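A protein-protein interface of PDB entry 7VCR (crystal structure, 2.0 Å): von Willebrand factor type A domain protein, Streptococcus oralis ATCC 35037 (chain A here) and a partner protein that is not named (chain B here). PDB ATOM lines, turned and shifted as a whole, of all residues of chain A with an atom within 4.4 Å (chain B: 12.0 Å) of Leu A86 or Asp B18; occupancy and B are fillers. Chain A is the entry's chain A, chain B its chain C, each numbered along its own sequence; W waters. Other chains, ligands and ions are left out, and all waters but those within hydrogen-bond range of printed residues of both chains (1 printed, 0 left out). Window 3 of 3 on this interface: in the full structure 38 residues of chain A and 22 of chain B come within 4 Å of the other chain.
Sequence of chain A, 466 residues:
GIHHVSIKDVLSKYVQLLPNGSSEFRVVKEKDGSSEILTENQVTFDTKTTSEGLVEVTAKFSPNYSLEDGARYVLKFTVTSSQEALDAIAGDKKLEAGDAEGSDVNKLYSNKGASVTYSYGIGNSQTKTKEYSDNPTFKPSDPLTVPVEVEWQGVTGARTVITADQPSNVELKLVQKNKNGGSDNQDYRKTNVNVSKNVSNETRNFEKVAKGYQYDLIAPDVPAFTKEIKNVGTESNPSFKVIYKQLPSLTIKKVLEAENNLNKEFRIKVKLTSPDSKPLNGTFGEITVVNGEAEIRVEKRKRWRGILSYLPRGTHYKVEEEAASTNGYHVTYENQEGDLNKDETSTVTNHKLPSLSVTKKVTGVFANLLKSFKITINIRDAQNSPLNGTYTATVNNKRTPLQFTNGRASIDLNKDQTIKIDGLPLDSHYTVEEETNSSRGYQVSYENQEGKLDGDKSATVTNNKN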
ATOM      1  N   VAL A  79     -17.178  11.038   8.352  1.00  0.00           N
ATOM      2  CA  VAL A  79     -16.246  11.121   7.241  1.00  0.00           C
ATOM      3  C   VAL A  79     -15.225  10.002   7.435  1.00  0.00           C
ATOM      4  O   VAL A  79     -15.161   9.406   8.517  1.00  0.00           O
ATOM      5  CB  VAL A  79     -15.537  12.468   7.158  1.00  0.00           C
ATOM      6  CG1 VAL A  79     -16.606  13.548   6.908  1.00  0.00           C
ATOM      7  CG2 VAL A  79     -14.736  12.807   8.415  1.00  0.00           C
ATOM      8  N   THR A  80     -14.447   9.735   6.371  1.00  0.00           N
ATOM      9  CA  THR A  80     -13.415   8.729   6.473  1.00  0.00           C
ATOM     10  C   THR A  80     -12.138   9.377   5.923  1.00  0.00           C
ATOM     11  O   THR A  80     -12.229  10.378   5.180  1.00  0.00           O
ATOM     12  CB  THR A  80     -13.914   7.465   5.746  1.00  0.00           C
ATOM     13  OG1 THR A  80     -12.940   6.473   6.113  1.00  0.00           O
ATOM     14  CG2 THR A  80     -13.888   7.647   4.232  1.00  0.00           C
ATOM     15  N   SER A  81     -10.952   8.892   6.341  1.00  0.00           N
ATOM     16  CA  SER A  81      -9.677   9.372   5.779  1.00  0.00           C
ATOM     17  C   SER A  81      -9.684   9.155   4.260  1.00  0.00           C
ATOM     18  O   SER A  81     -10.042   8.061   3.842  1.00  0.00           O
ATOM     19  CB  SER A  81      -8.550   8.478   6.356  1.00  0.00           C
ATOM     20  OG  SER A  81      -8.517   8.536   7.799  1.00  0.00           O
ATOM     21  N   SER A  82      -9.268  10.172   3.472  1.00  0.00           N
ATOM     22  CA  SER A  82      -9.136  10.101   2.051  1.00  0.00           C
ATOM     23  C   SER A  82      -7.815   9.374   1.760  1.00  0.00           C
ATOM     24  O   SER A  82      -6.990   9.209   2.662  1.00  0.00           O
ATOM     25  CB  SER A  82      -9.079  11.530   1.468  1.00  0.00           C
ATOM     26  OG  SER A  82      -7.830  12.141   1.891  1.00  0.00           O
ATOM     27  N   GLN A  83      -7.554   9.074   0.483  1.00  0.00           N
ATOM     28  CA  GLN A  83      -6.278   8.462   0.099  1.00  0.00           C
ATOM     29  C   GLN A  83      -5.132   9.381   0.501  1.00  0.00           C
ATOM     30  O   GLN A  83      -4.043   8.973   0.799  1.00  0.00           O
ATOM     31  CB  GLN A  83      -6.296   8.088  -1.416  1.00  0.00           C
ATOM     32  CG  GLN A  83      -5.066   7.179  -1.700  1.00  0.00           C
ATOM     33  CD  GLN A  83      -5.078   5.876  -0.889  1.00  0.00           C
ATOM     34  OE1 GLN A  83      -6.084   5.138  -0.879  1.00  0.00           O
ATOM     35  NE2 GLN A  83      -4.044   5.655  -0.062  1.00  0.00           N
ATOM     36  N   GLU A  84      -5.338  10.678   0.384  1.00  0.00           N
ATOM     37  CA  GLU A  84      -4.335  11.659   0.720  1.00  0.00           C
ATOM     38  C   GLU A  84      -3.893  11.512   2.180  1.00  0.00           C
ATOM     39  O   GLU A  84      -2.719  11.686   2.475  1.00  0.00           O
ATOM     40  CB  GLU A  84      -4.866  13.087   0.532  1.00  0.00           C
ATOM     41  CG  GLU A  84      -5.343  13.364  -0.866  1.00  0.00           C
ATOM     42  CD  GLU A  84      -4.325  14.161  -1.634  1.00  0.00           C
ATOM     43  OE1 GLU A  84      -3.203  14.369  -1.082  1.00  0.00           O
ATOM     44  OE2 GLU A  84      -4.661  14.566  -2.780  1.00  0.00           O
ATOM     45  N   ALA A  85      -4.828  11.278   3.099  1.00  0.00           N
ATOM     46  CA  ALA A  85      -4.476  11.139   4.510  1.00  0.00           C
ATOM     47  C   ALA A  85      -3.712   9.799   4.685  1.00  0.00           C
ATOM     48  O   ALA A  85      -2.779   9.724   5.475  1.00  0.00           O
ATOM     49  CB  ALA A  85      -5.765  11.175   5.351  1.00  0.00           C
ATOM     50  N   LEU A  86      -4.183   8.727   4.034  1.00  0.00           N
ATOM     51  CA  LEU A  86      -3.515   7.428   4.154  1.00  0.00           C
ATOM     52  C   LEU A  86      -2.101   7.490   3.579  1.00  0.00           C
ATOM     53  O   LEU A  86      -1.187   6.903   4.154  1.00  0.00           O
ATOM     54  CB  LEU A  86      -4.324   6.336   3.455  1.00  0.00           C
ATOM     55  CG  LEU A  86      -5.737   6.173   4.018  1.00  0.00           C
ATOM     56  CD1 LEU A  86      -6.539   5.192   3.185  1.00  0.00           C
ATOM     57  CD2 LEU A  86      -5.681   5.790   5.478  1.00  0.00           C
ATOM     58  N   ASP A  87      -1.912   8.261   2.498  1.00  0.00           N
ATOM     59  CA  ASP A  87      -0.577   8.436   1.913  1.00  0.00           C
ATOM     60  C   ASP A  87       0.332   9.200   2.875  1.00  0.00           C
ATOM     61  O   ASP A  87       1.482   8.810   3.059  1.00  0.00           O
ATOM     62  CB  ASP A  87      -0.617   9.163   0.557  1.00  0.00           C
ATOM     63  CG  ASP A  87      -1.234   8.354  -0.585  1.00  0.00           C
ATOM     64  OD1 ASP A  87      -1.398   7.139  -0.451  1.00  0.00           O
ATOM     65  OD2 ASP A  87      -1.636   8.963  -1.595  1.00  0.00           O
ATOM     66  N   ALA A  88      -0.153  10.349   3.406  1.00  0.00           N
ATOM     67  CA  ALA A  88       0.619  11.226   4.272  1.00  0.00           C
ATOM     68  C   ALA A  88       1.083  10.473   5.518  1.00  0.00           C
ATOM     69  O   ALA A  88       2.221  10.610   5.958  1.00  0.00           O
ATOM     70  CB  ALA A  88      -0.245  12.475   4.655  1.00  0.00           C
ATOM     71  N   ILE A  89       0.231   9.605   6.091  1.00  0.00           N
ATOM     72  CA  ILE A  89       0.670   8.940   7.310  1.00  0.00           C
ATOM     73  C   ILE A  89       1.697   7.815   7.027  1.00  0.00           C
ATOM     74  O   ILE A  89       2.480   7.474   7.904  1.00  0.00           O
ATOM     75  CB  ILE A  89      -0.512   8.431   8.135  1.00  0.00           C
ATOM     76  CG1 ILE A  89      -0.020   8.316   9.591  1.00  0.00           C
ATOM     77  CG2 ILE A  89      -1.121   7.153   7.525  1.00  0.00           C
ATOM     78  CD1 ILE A  89      -1.051   8.109  10.639  1.00  0.00           C
ATOM     79  N   ALA A  90       1.677   7.229   5.828  1.00  0.00           N
ATOM     80  CA  ALA A  90       2.699   6.266   5.380  1.00  0.00           C
ATOM     81  C   ALA A  90       3.988   7.005   5.017  1.00  0.00           C
ATOM     82  O   ALA A  90       4.963   6.359   4.681  1.00  0.00           O
ATOM     83  CB  ALA A  90       2.190   5.525   4.131  1.00  0.00           C
ATOM     84  N   PRO A 140      -5.059   9.744  11.065  1.00  0.00           N
ATOM     85  CA  PRO A 140      -5.495   8.557  10.326  1.00  0.00           C
ATOM     86  C   PRO A 140      -4.972   7.282  11.010  1.00  0.00           C
ATOM     87  O   PRO A 140      -4.120   7.371  11.869  1.00  0.00           O
ATOM     88  CB  PRO A 140      -4.661   8.691   9.012  1.00  0.00           C
ATOM     89  CG  PRO A 140      -4.368  10.187   8.910  1.00  0.00           C
ATOM     90  CD  PRO A 140      -4.099  10.601  10.347  1.00  0.00           C
ATOM     91  N   SER A 141      -5.481   6.100  10.648  1.00  0.00           N
ATOM     92  CA  SER A 141      -4.957   4.849  11.267  1.00  0.00           C
ATOM     93  C   SER A 141      -3.470   4.644  10.918  1.00  0.00           C
ATOM     94  O   SER A 141      -2.963   5.237   9.994  1.00  0.00           O
ATOM     95  CB  SER A 141      -5.709   3.644  10.785  1.00  0.00           C
ATOM     96  OG  SER A 141      -5.470   3.499   9.372  1.00  0.00           O
ATOM     97  N   ALA A 210       1.246   2.190   2.698  1.00  0.00           N
ATOM     98  CA  ALA A 210       0.007   2.963   2.748  1.00  0.00           C
ATOM     99  C   ALA A 210      -1.144   2.002   2.577  1.00  0.00           C
ATOM    100  O   ALA A 210      -1.099   1.174   1.652  1.00  0.00           O
ATOM    101  CB  ALA A 210       0.008   3.976   1.594  1.00  0.00           C
ATOM    102  N   LYS A 211      -2.220   2.191   3.378  1.00  0.00           N
ATOM    103  CA  LYS A 211      -3.479   1.506   3.137  1.00  0.00           C
ATOM    104  C   LYS A 211      -4.194   2.069   1.906  1.00  0.00           C
ATOM    105  O   LYS A 211      -3.891   3.198   1.436  1.00  0.00           O
ATOM    106  CB  LYS A 211      -4.381   1.742   4.375  1.00  0.00           C
ATOM    107  CG  LYS A 211      -3.969   0.873   5.531  1.00  0.00           C
ATOM    108  CD  LYS A 211      -4.793   0.992   6.728  1.00  0.00           C
ATOM    109  CE  LYS A 211      -4.267   0.141   7.869  1.00  0.00           C
ATOM    110  NZ  LYS A 211      -4.903   0.718   9.087  1.00  0.00           N
ATOM    111  N   ILE B  10     -14.452  16.977  15.968  1.00  0.00           N
ATOM    112  CA  ILE B  10     -14.390  15.704  15.246  1.00  0.00           C
ATOM    113  C   ILE B  10     -14.002  14.622  16.253  1.00  0.00           C
ATOM    114  O   ILE B  10     -13.231  14.874  17.149  1.00  0.00           O
ATOM    115  CB  ILE B  10     -13.423  15.813  14.066  1.00  0.00           C
ATOM    116  CG1 ILE B  10     -13.644  14.661  13.082  1.00  0.00           C
ATOM    117  CG2 ILE B  10     -11.979  15.902  14.580  1.00  0.00           C
ATOM    118  CD1 ILE B  10     -12.795  14.642  11.800  1.00  0.00           C
ATOM    119  N   THR B  11     -14.629  13.446  16.177  1.00  0.00           N
ATOM    120  CA  THR B  11     -14.420  12.389  17.143  1.00  0.00           C
ATOM    121  C   THR B  11     -14.178  11.075  16.384  1.00  0.00           C
ATOM    122  O   THR B  11     -15.043  10.688  15.630  1.00  0.00           O
ATOM    123  CB  THR B  11     -15.677  12.149  17.989  1.00  0.00           C
ATOM    124  OG1 THR B  11     -15.837  13.449  18.573  1.00  0.00           O
ATOM    125  CG2 THR B  11     -15.450  11.180  19.163  1.00  0.00           C
ATOM    126  N   PRO B  12     -13.055  10.349  16.560  1.00  0.00           N
ATOM    127  CA  PRO B  12     -12.889   9.008  15.966  1.00  0.00           C
ATOM    128  C   PRO B  12     -14.056   8.108  16.371  1.00  0.00           C
ATOM    129  O   PRO B  12     -14.558   8.270  17.449  1.00  0.00           O
ATOM    130  CB  PRO B  12     -11.627   8.384  16.656  1.00  0.00           C
ATOM    131  CG  PRO B  12     -10.860   9.629  17.107  1.00  0.00           C
ATOM    132  CD  PRO B  12     -11.913  10.724  17.420  1.00  0.00           C
ATOM    133  N   ILE B  13     -14.564   7.275  15.475  1.00  0.00           N
ATOM    134  CA  ILE B  13     -15.618   6.352  15.852  1.00  0.00           C
ATOM    135  C   ILE B  13     -14.918   5.093  16.406  1.00  0.00           C
ATOM    136  O   ILE B  13     -14.097   4.469  15.734  1.00  0.00           O
ATOM    137  CB  ILE B  13     -16.554   6.068  14.659  1.00  0.00           C
ATOM    138  CG1 ILE B  13     -17.405   7.303  14.353  1.00  0.00           C
ATOM    139  CG2 ILE B  13     -17.493   4.914  14.996  1.00  0.00           C
ATOM    140  CD1 ILE B  13     -18.066   7.247  13.018  1.00  0.00           C
ATOM    141  N   SER B  14     -15.134   4.820  17.688  1.00  0.00           N
ATOM    142  CA  SER B  14     -14.513   3.699  18.375  1.00  0.00           C
ATOM    143  C   SER B  14     -14.685   2.367  17.590  1.00  0.00           C
ATOM    144  O   SER B  14     -15.763   2.005  17.158  1.00  0.00           O
ATOM    145  CB  SER B  14     -15.103   3.700  19.792  1.00  0.00           C
ATOM    146  OG  SER B  14     -14.950   2.436  20.405  1.00  0.00           O
ATOM    147  N   GLY B  15     -13.590   1.636  17.398  1.00  0.00           N
ATOM    148  CA  GLY B  15     -13.544   0.311  16.781  1.00  0.00           C
ATOM    149  C   GLY B  15     -13.750   0.377  15.269  1.00  0.00           C
ATOM    150  O   GLY B  15     -14.103  -0.633  14.704  1.00  0.00           O
ATOM    151  N   GLN B  16     -13.671   1.578  14.636  1.00  0.00           N
ATOM    152  CA  GLN B  16     -13.726   1.623  13.179  1.00  0.00           C
ATOM    153  C   GLN B  16     -12.594   2.509  12.678  1.00  0.00           C
ATOM    154  O   GLN B  16     -12.720   3.747  12.626  1.00  0.00           O
ATOM    155  CB  GLN B  16     -15.033   2.263  12.714  1.00  0.00           C
ATOM    156  CG  GLN B  16     -16.256   1.477  13.098  1.00  0.00           C
ATOM    157  CD  GLN B  16     -17.537   1.998  12.508  1.00  0.00           C
ATOM    158  OE1 GLN B  16     -17.670   2.225  11.294  1.00  0.00           O
ATOM    159  NE2 GLN B  16     -18.531   2.083  13.359  1.00  0.00           N
ATOM    160  N   ASP B  17     -11.551   1.881  12.160  1.00  0.00           N
ATOM    161  CA  ASP B  17     -10.374   2.554  11.642  1.00  0.00           C
ATOM    162  C   ASP B  17     -10.764   3.620  10.608  1.00  0.00           C
ATOM    163  O   ASP B  17     -11.570   3.374   9.716  1.00  0.00           O
ATOM    164  CB  ASP B  17      -9.466   1.564  10.887  1.00  0.00           C
ATOM    165  CG  ASP B  17      -8.667   0.632  11.804  1.00  0.00           C
ATOM    166  OD1 ASP B  17      -8.738   0.798  13.065  1.00  0.00           O
ATOM    167  OD2 ASP B  17      -7.953  -0.268  11.242  1.00  0.00           O
ATOM    168  N   ASP B  18     -10.115   4.767  10.703  1.00  0.00           N
ATOM    169  CA  ASP B  18     -10.228   5.787   9.653  1.00  0.00           C
ATOM    170  C   ASP B  18     -11.669   6.370   9.578  1.00  0.00           C
ATOM    171  O   ASP B  18     -11.999   6.971   8.533  1.00  0.00           O
ATOM    172  CB  ASP B  18      -9.711   5.253   8.284  1.00  0.00           C
ATOM    173  CG  ASP B  18      -8.188   5.106   8.358  1.00  0.00           C
ATOM    174  OD1 ASP B  18      -7.514   6.163   8.610  1.00  0.00           O
ATOM    175  OD2 ASP B  18      -7.653   3.871   8.314  1.00  0.00           O
ATOM    176  N   LYS B  19     -12.529   6.164  10.610  1.00  0.00           N
ATOM    177  CA  LYS B  19     -13.853   6.791  10.552  1.00  0.00           C
ATOM    178  C   LYS B  19     -14.012   7.802  11.709  1.00  0.00           C
ATOM    179  O   LYS B  19     -13.517   7.561  12.813  1.00  0.00           O
ATOM    180  CB  LYS B  19     -15.030   5.825  10.600  1.00  0.00           C
ATOM    181  CG  LYS B  19     -15.018   4.780   9.490  1.00  0.00           C
ATOM    182  CD  LYS B  19     -16.344   4.560   8.833  1.00  0.00           C
ATOM    183  CE  LYS B  19     -16.251   3.582   7.667  1.00  0.00           C
ATOM    184  NZ  LYS B  19     -14.919   3.702   7.004  1.00  0.00           N
ATOM    185  N   TYR B  20     -14.652   8.958  11.427  1.00  0.00           N
ATOM    186  CA  TYR B  20     -14.691  10.082  12.383  1.00  0.00           C
ATOM    187  C   TYR B  20     -16.056  10.739  12.231  1.00  0.00           C
ATOM    188  O   TYR B  20     -16.610  10.763  11.136  1.00  0.00           O
ATOM    189  CB  TYR B  20     -13.635  11.178  12.102  1.00  0.00           C
ATOM    190  CG  TYR B  20     -12.253  10.609  11.908  1.00  0.00           C
ATOM    191  CD1 TYR B  20     -11.933   9.980  10.700  1.00  0.00           C
ATOM    192  CD2 TYR B  20     -11.380  10.491  12.985  1.00  0.00           C
ATOM    193  CE1 TYR B  20     -10.693   9.396  10.523  1.00  0.00           C
ATOM    194  CE2 TYR B  20     -10.153   9.869  12.830  1.00  0.00           C
ATOM    195  CZ  TYR B  20      -9.839   9.279  11.590  1.00  0.00           C
ATOM    196  OH  TYR B  20      -8.661   8.587  11.345  1.00  0.00           O
ATOM    197  N   GLU B  21     -16.625  11.199  13.353  1.00  0.00           N
ATOM    198  CA  GLU B  21     -17.912  11.883  13.291  1.00  0.00           C
ATOM    199  C   GLU B  21     -17.651  13.380  13.471  1.00  0.00           C
ATOM    200  O   GLU B  21     -16.978  13.788  14.435  1.00  0.00           O
ATOM    201  CB  GLU B  21     -18.815  11.374  14.425  1.00  0.00           C
ATOM    202  CG  GLU B  21     -20.116  12.175  14.375  1.00  0.00           C
ATOM    203  CD  GLU B  21     -21.184  11.478  15.182  1.00  0.00           C
ATOM    204  OE1 GLU B  21     -21.183  11.758  16.413  1.00  0.00           O
ATOM    205  OE2 GLU B  21     -21.978  10.643  14.605  1.00  0.00           O
ATOM    206  N   LEU B  22     -18.090  14.172  12.516  1.00  0.00           N
ATOM    207  CA  LEU B  22     -18.015  15.630  12.654  1.00  0.00           C
ATOM    208  C   LEU B  22     -19.311  16.098  13.316  1.00  0.00           C
ATOM    209  O   LEU B  22     -20.422  15.575  13.004  1.00  0.00           O
ATOM    210  CB  LEU B  22     -17.899  16.313  11.268  1.00  0.00           C
ATOM    211  CG  LEU B  22     -16.427  16.387  10.815  1.00  0.00           C
ATOM    212  CD1 LEU B  22     -16.287  16.645   9.296  1.00  0.00           C
ATOM    213  CD2 LEU B  22     -15.782  17.552  11.580  1.00  0.00           C
HETATM  214  O   HOH W   1      -7.209  -0.121   8.847  1.00  0.00           O
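The side-chain carboxylate of Asp B18 is in hydrogen-bond range of the side-chain hydroxyl of Ser A141, 2.5 Å away. O of Asp B18 sits at hydrogen-bond distance from OG1 of Thr A80 (2.6 Å). OD1 of Asp B18 lies within hydrogen-bond range of OG of Ser A81 (2.7 Å). NZ of Lys A211 lies within salt-bridge range of OD2 of Asp B17 (3.9 Å). O of Tyr B20 lies within hydrogen-bond range of N of Val A79 (2.9 Å).
The backbone NH (N) of Ile B13 is in hydrogen-bond range of the backbone carbonyl oxygen (O) of Lys B19 (2.9 Å). O of Lys A211 sits at hydrogen-bond distance from NE2 of Gln A83, 2.9 Å away. The side-chain amino group (NZ) of Lys A211 sits at hydrogen-bond distance from the side-chain hydroxyl (OG) of Ser A141, at 2.9 Å.
O of Val A79 touches O of Asp B18 (3.99 Å). Val A79 touches Lys B19 (O to CA, 3.6 Å). Leu B22 touches Val A79 (CD1 to CG1, 3.9 Å). Lys B19 touches Thr A80 (NZ to OG1, 3.5 Å). Tyr B20 touches Ser A81. OD1 of Asp B18 touches CD2 of Leu A86 (3.6 Å). Asp B18 touches Pro A140. Tyr B20 touches Pro A140.
Of the printed residues of chain B, Val A79 touches Asp B18, Lys B19, Tyr B20 and Leu B22. Thr A80 touches two residues of chain B. Ser A81 touches two residues of chain B. No residue of chain B comes within 4 Å of Ser A82. Glu A84 touches none of the printed residues of chain B. No residue of chain B comes within 4 Å of Ala A85. Leu A86 touches just one residue of chain B: Asp B18 (3.6 Å). No residue of chain B comes within 4 Å of Ala A88. No residue of chain B comes within 4 Å of Ile A89. Of chain B, only Asp B18 (3.6 Å) and Tyr B20 (3.3 Å) come within 4 Å of Pro A140. Printed residues of chain B within 4 Å of Ser A141: Asp B18 (2.5 Å). Of chain B, only Asp B17 (3.9 Å) comes within 4 Å of Lys A211. Gln B16 touches none of the printed residues of chain A. Of the printed residues of chain A, Asp B17 touches Lys A211 (3.9 Å). Of the printed residues of chain A, Asp B18 touches Val A79, Thr A80, Ser A81, Leu A86, Pro A140 and Ser A141. Of the printed residues of chain A, Lys B19 touches Val A79 (3.6 Å) and Thr A80 (3.5 Å). Printed residues of chain A within 4 Å of Tyr B20: Val A79 (2.9 Å), Ser A81 (3.5 Å) and Pro A140 (3.3 Å). Of the printed residues of chain A, Leu B22 touches Val A79 (3.9 Å). The nearest residue of chain B that does not touch Leu A86 is Tyr B20 (7.2 Å). The nearest printed residue of chain A that does not touch Asp B18 is Lys A211 (4.3 Å). The nearest printed residue of chain A that does not touch Asp B17 is Ser A141 (4.3 Å).
Hydrophobic or aromatic side chains of chain A that line the printed part of chain B: Val A79, Leu A86 and Pro A140. Printed residues of chain B that touch a printed residue of chain A: Asp B17, Asp B18, Lys B19, Tyr B20 and Leu B22. Hydrophobic or aromatic side chains of chain B that line the printed part of chain A: Tyr B20 and Leu B22. Among the printed residues, 13 pairs touch across the chains. Among the printed residues, Asp or Glu carboxylates within 4 Å of a Lys or Arg side-chain nitrogen of the other chain: Lys A211 with Asp B17 (3.9 Å).
Water W1 lies within hydrogen-bond range of the side-chain amino group (NZ) of Lys A211 (2.5 Å) and the side-chain carboxylate (OD2) of Asp B17 (2.5 Å).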
